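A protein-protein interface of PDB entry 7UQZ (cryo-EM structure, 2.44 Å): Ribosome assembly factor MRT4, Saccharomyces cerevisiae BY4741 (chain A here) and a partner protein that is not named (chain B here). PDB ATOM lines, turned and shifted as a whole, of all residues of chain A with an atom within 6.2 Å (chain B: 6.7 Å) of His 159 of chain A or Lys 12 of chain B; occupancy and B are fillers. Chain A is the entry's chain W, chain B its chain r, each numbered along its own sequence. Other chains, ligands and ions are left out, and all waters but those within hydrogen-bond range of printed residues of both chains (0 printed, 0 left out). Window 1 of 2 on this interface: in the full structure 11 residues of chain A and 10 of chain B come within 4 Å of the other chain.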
ATOM      1  N   MET A 157      29.177 -20.160  16.451  1.00  0.00           N
ATOM      2  CA  MET A 157      28.498 -20.330  17.728  1.00  0.00           C
ATOM      3  C   MET A 157      27.014 -20.014  17.588  1.00  0.00           C
ATOM      4  O   MET A 157      26.628 -19.042  16.935  1.00  0.00           O
ATOM      5  CB  MET A 157      29.134 -19.425  18.784  1.00  0.00           C
ATOM      6  CG  MET A 157      28.639 -19.663  20.200  1.00  0.00           C
ATOM      7  SD  MET A 157      29.383 -21.114  20.963  1.00  0.00           S
ATOM      8  CE  MET A 157      30.992 -20.473  21.410  1.00  0.00           C
ATOM      9  N   ILE A 158      26.180 -20.854  18.203  1.00  0.00           N
ATOM     10  CA  ILE A 158      24.734 -20.701  18.089  1.00  0.00           C
ATOM     11  C   ILE A 158      24.295 -19.429  18.805  1.00  0.00           C
ATOM     12  O   ILE A 158      24.843 -19.058  19.852  1.00  0.00           O
ATOM     13  CB  ILE A 158      24.026 -21.956  18.636  1.00  0.00           C
ATOM     14  CG1 ILE A 158      22.509 -21.862  18.458  1.00  0.00           C
ATOM     15  CG2 ILE A 158      24.397 -22.205  20.088  1.00  0.00           C
ATOM     16  CD1 ILE A 158      22.072 -21.753  17.015  1.00  0.00           C
ATOM     17  N   HIS A 159      23.311 -18.736  18.221  1.00  0.00           N
ATOM     18  CA  HIS A 159      22.878 -17.440  18.736  1.00  0.00           C
ATOM     19  C   HIS A 159      22.252 -17.530  20.123  1.00  0.00           C
ATOM     20  O   HIS A 159      22.199 -16.517  20.828  1.00  0.00           O
ATOM     21  CB  HIS A 159      21.886 -16.805  17.764  1.00  0.00           C
ATOM     22  CG  HIS A 159      20.674 -17.643  17.510  1.00  0.00           C
ATOM     23  ND1 HIS A 159      20.656 -18.660  16.581  1.00  0.00           N
ATOM     24  CD2 HIS A 159      19.441 -17.623  18.070  1.00  0.00           C
ATOM     25  CE1 HIS A 159      19.464 -19.230  16.578  1.00  0.00           C
ATOM     26  NE2 HIS A 159      18.709 -18.619  17.472  1.00  0.00           N
ATOM     27  N   SER A 160      21.781 -18.709  20.533  1.00  0.00           N
ATOM     28  CA  SER A 160      21.151 -18.848  21.842  1.00  0.00           C
ATOM     29  C   SER A 160      22.143 -18.723  22.992  1.00  0.00           C
ATOM     30  O   SER A 160      21.722 -18.491  24.131  1.00  0.00           O
ATOM     31  CB  SER A 160      20.422 -20.189  21.937  1.00  0.00           C
ATOM     32  OG  SER A 160      19.369 -20.265  20.994  1.00  0.00           O
ATOM     33  N   LEU A 161      23.439 -18.873  22.729  1.00  0.00           N
ATOM     34  CA  LEU A 161      24.455 -18.774  23.767  1.00  0.00           C
ATOM     35  C   LEU A 161      24.967 -17.356  23.973  1.00  0.00           C
ATOM     36  O   LEU A 161      25.810 -17.143  24.850  1.00  0.00           O
ATOM     37  CB  LEU A 161      25.635 -19.697  23.443  1.00  0.00           C
ATOM     38  CG  LEU A 161      25.379 -21.201  23.535  1.00  0.00           C
ATOM     39  CD1 LEU A 161      26.638 -21.973  23.189  1.00  0.00           C
ATOM     40  CD2 LEU A 161      24.882 -21.576  24.920  1.00  0.00           C
ATOM     41  N   GLU A 162      24.498 -16.393  23.183  1.00  0.00           N
ATOM     42  CA  GLU A 162      24.980 -15.021  23.330  1.00  0.00           C
ATOM     43  C   GLU A 162      24.627 -14.381  24.671  1.00  0.00           C
ATOM     44  O   GLU A 162      25.502 -13.700  25.234  1.00  0.00           O
ATOM     45  CB  GLU A 162      24.488 -14.165  22.155  1.00  0.00           C
ATOM     46  CG  GLU A 162      25.252 -12.862  21.982  1.00  0.00           C
ATOM     47  CD  GLU A 162      24.657 -11.719  22.778  1.00  0.00           C
ATOM     48  OE1 GLU A 162      23.468 -11.810  23.151  1.00  0.00           O
ATOM     49  OE2 GLU A 162      25.375 -10.732  23.034  1.00  0.00           O
ATOM     50  N   PRO A 163      23.406 -14.504  25.218  1.00  0.00           N
ATOM     51  CA  PRO A 163      23.195 -13.993  26.586  1.00  0.00           C
ATOM     52  C   PRO A 163      24.086 -14.654  27.624  1.00  0.00           C
ATOM     53  O   PRO A 163      24.532 -13.985  28.563  1.00  0.00           O
ATOM     54  CB  PRO A 163      21.711 -14.286  26.842  1.00  0.00           C
ATOM     55  CG  PRO A 163      21.105 -14.295  25.505  1.00  0.00           C
ATOM     56  CD  PRO A 163      22.126 -14.918  24.610  1.00  0.00           C
ATOM     57  N   ILE A 175      25.184  -9.419  18.550  1.00  0.00           N
ATOM     58  CA  ILE A 175      24.511 -10.274  17.581  1.00  0.00           C
ATOM     59  C   ILE A 175      24.422  -9.499  16.277  1.00  0.00           C
ATOM     60  O   ILE A 175      23.717  -8.486  16.193  1.00  0.00           O
ATOM     61  CB  ILE A 175      23.120 -10.706  18.065  1.00  0.00           C
ATOM     62  CG1 ILE A 175      23.217 -11.355  19.443  1.00  0.00           C
ATOM     63  CG2 ILE A 175      22.487 -11.666  17.072  1.00  0.00           C
ATOM     64  CD1 ILE A 175      21.915 -11.923  19.950  1.00  0.00           C
ATOM     65  N   ALA A 177      23.391 -10.277  12.410  1.00  0.00           N
ATOM     66  CA  ALA A 177      22.769 -11.199  11.454  1.00  0.00           C
ATOM     67  C   ALA A 177      22.685 -12.618  12.014  1.00  0.00           C
ATOM     68  O   ALA A 177      22.893 -13.604  11.306  1.00  0.00           O
ATOM     69  CB  ALA A 177      23.506 -11.183  10.113  1.00  0.00           C
ATOM     70  N   GLY A 178      22.376 -12.720  13.304  1.00  0.00           N
ATOM     71  CA  GLY A 178      22.274 -14.016  13.941  1.00  0.00           C
ATOM     72  C   GLY A 178      23.592 -14.681  14.259  1.00  0.00           C
ATOM     73  O   GLY A 178      23.612 -15.887  14.524  1.00  0.00           O
ATOM     74  N   LYS A 179      24.696 -13.940  14.235  1.00  0.00           N
ATOM     75  CA  LYS A 179      26.010 -14.484  14.542  1.00  0.00           C
ATOM     76  C   LYS A 179      26.644 -13.698  15.681  1.00  0.00           C
ATOM     77  O   LYS A 179      26.522 -12.471  15.744  1.00  0.00           O
ATOM     78  CB  LYS A 179      26.918 -14.460  13.309  1.00  0.00           C
ATOM     79  CG  LYS A 179      26.420 -15.331  12.169  1.00  0.00           C
ATOM     80  CD  LYS A 179      27.397 -15.343  11.010  1.00  0.00           C
ATOM     81  CE  LYS A 179      26.962 -16.323   9.936  1.00  0.00           C
ATOM     82  NZ  LYS A 179      27.956 -16.398   8.829  1.00  0.00           N
ATOM     83  N   ILE A 180      27.313 -14.414  16.579  1.00  0.00           N
ATOM     84  CA  ILE A 180      27.961 -13.799  17.732  1.00  0.00           C
ATOM     85  C   ILE A 180      29.290 -13.200  17.295  1.00  0.00           C
ATOM     86  O   ILE A 180      30.128 -13.882  16.696  1.00  0.00           O
ATOM     87  CB  ILE A 180      28.156 -14.828  18.857  1.00  0.00           C
ATOM     88  CG1 ILE A 180      26.813 -15.451  19.244  1.00  0.00           C
ATOM     89  CG2 ILE A 180      28.819 -14.185  20.062  1.00  0.00           C
ATOM     90  CD1 ILE A 180      26.891 -16.394  20.423  1.00  0.00           C
ATOM     91  N   ASP B   5       6.691 -15.600  10.298  1.00  0.00           N
ATOM     92  CA  ASP B   5       7.071 -15.415  11.701  1.00  0.00           C
ATOM     93  C   ASP B   5       8.221 -14.410  11.808  1.00  0.00           C
ATOM     94  O   ASP B   5       9.356 -14.728  12.177  1.00  0.00           O
ATOM     95  CB  ASP B   5       7.422 -16.756  12.334  1.00  0.00           C
ATOM     96  CG  ASP B   5       8.466 -17.519  11.545  1.00  0.00           C
ATOM     97  OD1 ASP B   5       8.508 -17.370  10.306  1.00  0.00           O
ATOM     98  OD2 ASP B   5       9.249 -18.266  12.167  1.00  0.00           O
ATOM     99  N   ILE B   7       8.650 -11.802  13.841  1.00  0.00           N
ATOM    100  CA  ILE B   7       9.143 -11.480  15.178  1.00  0.00           C
ATOM    101  C   ILE B   7      10.117 -12.548  15.660  1.00  0.00           C
ATOM    102  O   ILE B   7      11.161 -12.236  16.247  1.00  0.00           O
ATOM    103  CB  ILE B   7       7.965 -11.292  16.154  1.00  0.00           C
ATOM    104  CG1 ILE B   7       7.211  -9.998  15.840  1.00  0.00           C
ATOM    105  CG2 ILE B   7       8.438 -11.297  17.601  1.00  0.00           C
ATOM    106  CD1 ILE B   7       8.052  -8.750  15.971  1.00  0.00           C
ATOM    107  N   GLU B   8       9.800 -13.821  15.417  1.00  0.00           N
ATOM    108  CA  GLU B   8      10.731 -14.889  15.764  1.00  0.00           C
ATOM    109  C   GLU B   8      12.010 -14.793  14.944  1.00  0.00           C
ATOM    110  O   GLU B   8      13.108 -15.020  15.465  1.00  0.00           O
ATOM    111  CB  GLU B   8      10.068 -16.253  15.582  1.00  0.00           C
ATOM    112  CG  GLU B   8       9.303 -16.722  16.807  1.00  0.00           C
ATOM    113  CD  GLU B   8       8.565 -18.026  16.576  1.00  0.00           C
ATOM    114  OE1 GLU B   8       8.439 -18.444  15.406  1.00  0.00           O
ATOM    115  OE2 GLU B   8       8.109 -18.633  17.566  1.00  0.00           O
ATOM    116  N   ARG B   9      11.893 -14.442  13.659  1.00  0.00           N
ATOM    117  CA  ARG B   9      13.090 -14.233  12.849  1.00  0.00           C
ATOM    118  C   ARG B   9      13.915 -13.061  13.369  1.00  0.00           C
ATOM    119  O   ARG B   9      15.149 -13.108  13.356  1.00  0.00           O
ATOM    120  CB  ARG B   9      12.713 -14.012  11.385  1.00  0.00           C
ATOM    121  CG  ARG B   9      12.187 -15.254  10.686  1.00  0.00           C
ATOM    122  CD  ARG B   9      12.200 -15.089   9.176  1.00  0.00           C
ATOM    123  NE  ARG B   9      11.473 -13.902   8.742  1.00  0.00           N
ATOM    124  CZ  ARG B   9      10.189 -13.889   8.415  1.00  0.00           C
ATOM    125  NH1 ARG B   9       9.450 -14.983   8.474  1.00  0.00           N
ATOM    126  NH2 ARG B   9       9.634 -12.749   8.015  1.00  0.00           N
ATOM    127  N   HIS B  10      13.251 -11.998  13.827  1.00  0.00           N
ATOM    128  CA  HIS B  10      13.960 -10.845  14.372  1.00  0.00           C
ATOM    129  C   HIS B  10      14.680 -11.202  15.665  1.00  0.00           C
ATOM    130  O   HIS B  10      15.792 -10.728  15.912  1.00  0.00           O
ATOM    131  CB  HIS B  10      12.985  -9.691  14.603  1.00  0.00           C
ATOM    132  CG  HIS B  10      13.643  -8.431  15.069  1.00  0.00           C
ATOM    133  ND1 HIS B  10      14.154  -7.493  14.199  1.00  0.00           N
ATOM    134  CD2 HIS B  10      13.880  -7.956  16.314  1.00  0.00           C
ATOM    135  CE1 HIS B  10      14.673  -6.493  14.887  1.00  0.00           C
ATOM    136  NE2 HIS B  10      14.521  -6.749  16.173  1.00  0.00           N
ATOM    137  N   ILE B  11      14.053 -12.022  16.509  1.00  0.00           N
ATOM    138  CA  ILE B  11      14.714 -12.497  17.721  1.00  0.00           C
ATOM    139  C   ILE B  11      15.910 -13.374  17.364  1.00  0.00           C
ATOM    140  O   ILE B  11      16.966 -13.305  18.003  1.00  0.00           O
ATOM    141  CB  ILE B  11      13.704 -13.236  18.620  1.00  0.00           C
ATOM    142  CG1 ILE B  11      12.655 -12.258  19.152  1.00  0.00           C
ATOM    143  CG2 ILE B  11      14.405 -13.937  19.771  1.00  0.00           C
ATOM    144  CD1 ILE B  11      11.569 -12.911  19.975  1.00  0.00           C
ATOM    145  N   LYS B  12      15.765 -14.198  16.326  1.00  0.00           N
ATOM    146  CA  LYS B  12      16.845 -15.092  15.921  1.00  0.00           C
ATOM    147  C   LYS B  12      18.022 -14.322  15.330  1.00  0.00           C
ATOM    148  O   LYS B  12      19.181 -14.710  15.517  1.00  0.00           O
ATOM    149  CB  LYS B  12      16.305 -16.111  14.918  1.00  0.00           C
ATOM    150  CG  LYS B  12      17.129 -17.371  14.770  1.00  0.00           C
ATOM    151  CD  LYS B  12      16.377 -18.407  13.944  1.00  0.00           C
ATOM    152  CE  LYS B  12      15.019 -18.716  14.560  1.00  0.00           C
ATOM    153  NZ  LYS B  12      14.174 -19.572  13.682  1.00  0.00           N
ATOM    154  N   GLN B  13      17.746 -13.230  14.618  1.00  0.00           N
ATOM    155  CA  GLN B  13      18.782 -12.496  13.897  1.00  0.00           C
ATOM    156  C   GLN B  13      19.373 -11.333  14.684  1.00  0.00           C
ATOM    157  O   GLN B  13      20.509 -10.930  14.411  1.00  0.00           O
ATOM    158  CB  GLN B  13      18.219 -11.971  12.574  1.00  0.00           C
ATOM    159  CG  GLN B  13      17.929 -13.052  11.552  1.00  0.00           C
ATOM    160  CD  GLN B  13      19.170 -13.492  10.807  1.00  0.00           C
ATOM    161  OE1 GLN B  13      19.941 -12.665  10.324  1.00  0.00           O
ATOM    162  NE2 GLN B  13      19.372 -14.800  10.710  1.00  0.00           N
ATOM    163  N   HIS B  14      18.638 -10.775  15.647  1.00  0.00           N
ATOM    164  CA  HIS B  14      19.088  -9.607  16.388  1.00  0.00           C
ATOM    165  C   HIS B  14      19.062  -9.784  17.897  1.00  0.00           C
ATOM    166  O   HIS B  14      19.601  -8.929  18.608  1.00  0.00           O
ATOM    167  CB  HIS B  14      18.236  -8.378  16.025  1.00  0.00           C
ATOM    168  CG  HIS B  14      18.112  -8.139  14.553  1.00  0.00           C
ATOM    169  ND1 HIS B  14      19.044  -7.424  13.834  1.00  0.00           N
ATOM    170  CD2 HIS B  14      17.162  -8.517  13.666  1.00  0.00           C
ATOM    171  CE1 HIS B  14      18.677  -7.374  12.567  1.00  0.00           C
ATOM    172  NE2 HIS B  14      17.538  -8.030  12.438  1.00  0.00           N
ATOM    173  N   GLY B  15      18.464 -10.854  18.407  1.00  0.00           N
ATOM    174  CA  GLY B  15      18.343 -11.035  19.836  1.00  0.00           C
ATOM    175  C   GLY B  15      17.226 -10.201  20.433  1.00  0.00           C
ATOM    176  O   GLY B  15      16.350  -9.672  19.744  1.00  0.00           O
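Printed residues of chain A that touch a printed residue of chain B: His 159, Ile 175, Ala 177 and Gly 178.
Hydrophobic or aromatic side chains of chain A that line the printed part of chain B: His 159, Ile 175 and Ala 177.
Printed residues of chain B within 4 Å of His 159 of chain A: Lys 12.
Of chain A, only His 159 (3.4 Å) and Gly 178 (3.5 Å) come within 4 Å of Lys 12 of chain B.
Printed residues of chain A within 4 Å of His 14 of chain B: Ile 175.
Of the printed residues of chain B, Gly 178 of chain A touches Lys 12 (3.5 Å) and Gln 13 (2.8 Å).
Of the printed residues of chain B, Ile 175 of chain A touches Gln 13, His 14 and Gly 15.
Of the printed residues of chain A, Gly 15 of chain B touches Ile 175.
Of the printed residues of chain A, Gln 13 of chain B touches Ile 175, Ala 177 and Gly 178.
The nearest residue of chain A that does not touch Lys 12 of chain B is Ile 175 of chain A (4.8 Å).
The backbone carbonyl oxygen (O) of Ala 177 of chain A sits close to the side-chain amide oxygen (OE1) of Gln 13 of chain B (3.2 Å).
The backbone NH (N) of Gly 178 of chain A sits at hydrogen-bond distance from the backbone carbonyl oxygen (O) of Gln 13 of chain B.
His 159 of chain A touches Lys 12 of chain B (NE2 to CG, 3.4 Å).
Ile 175 of chain A touches Gln 13 of chain B.
CB of Ile 175 of chain A touches O of His 14 of chain B, at 3.98 Å.
Ile 175 of chain A touches Gly 15 of chain B (CD1 to CA, 3.7 Å).
Gly 178 of chain A touches Lys 12 of chain B.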
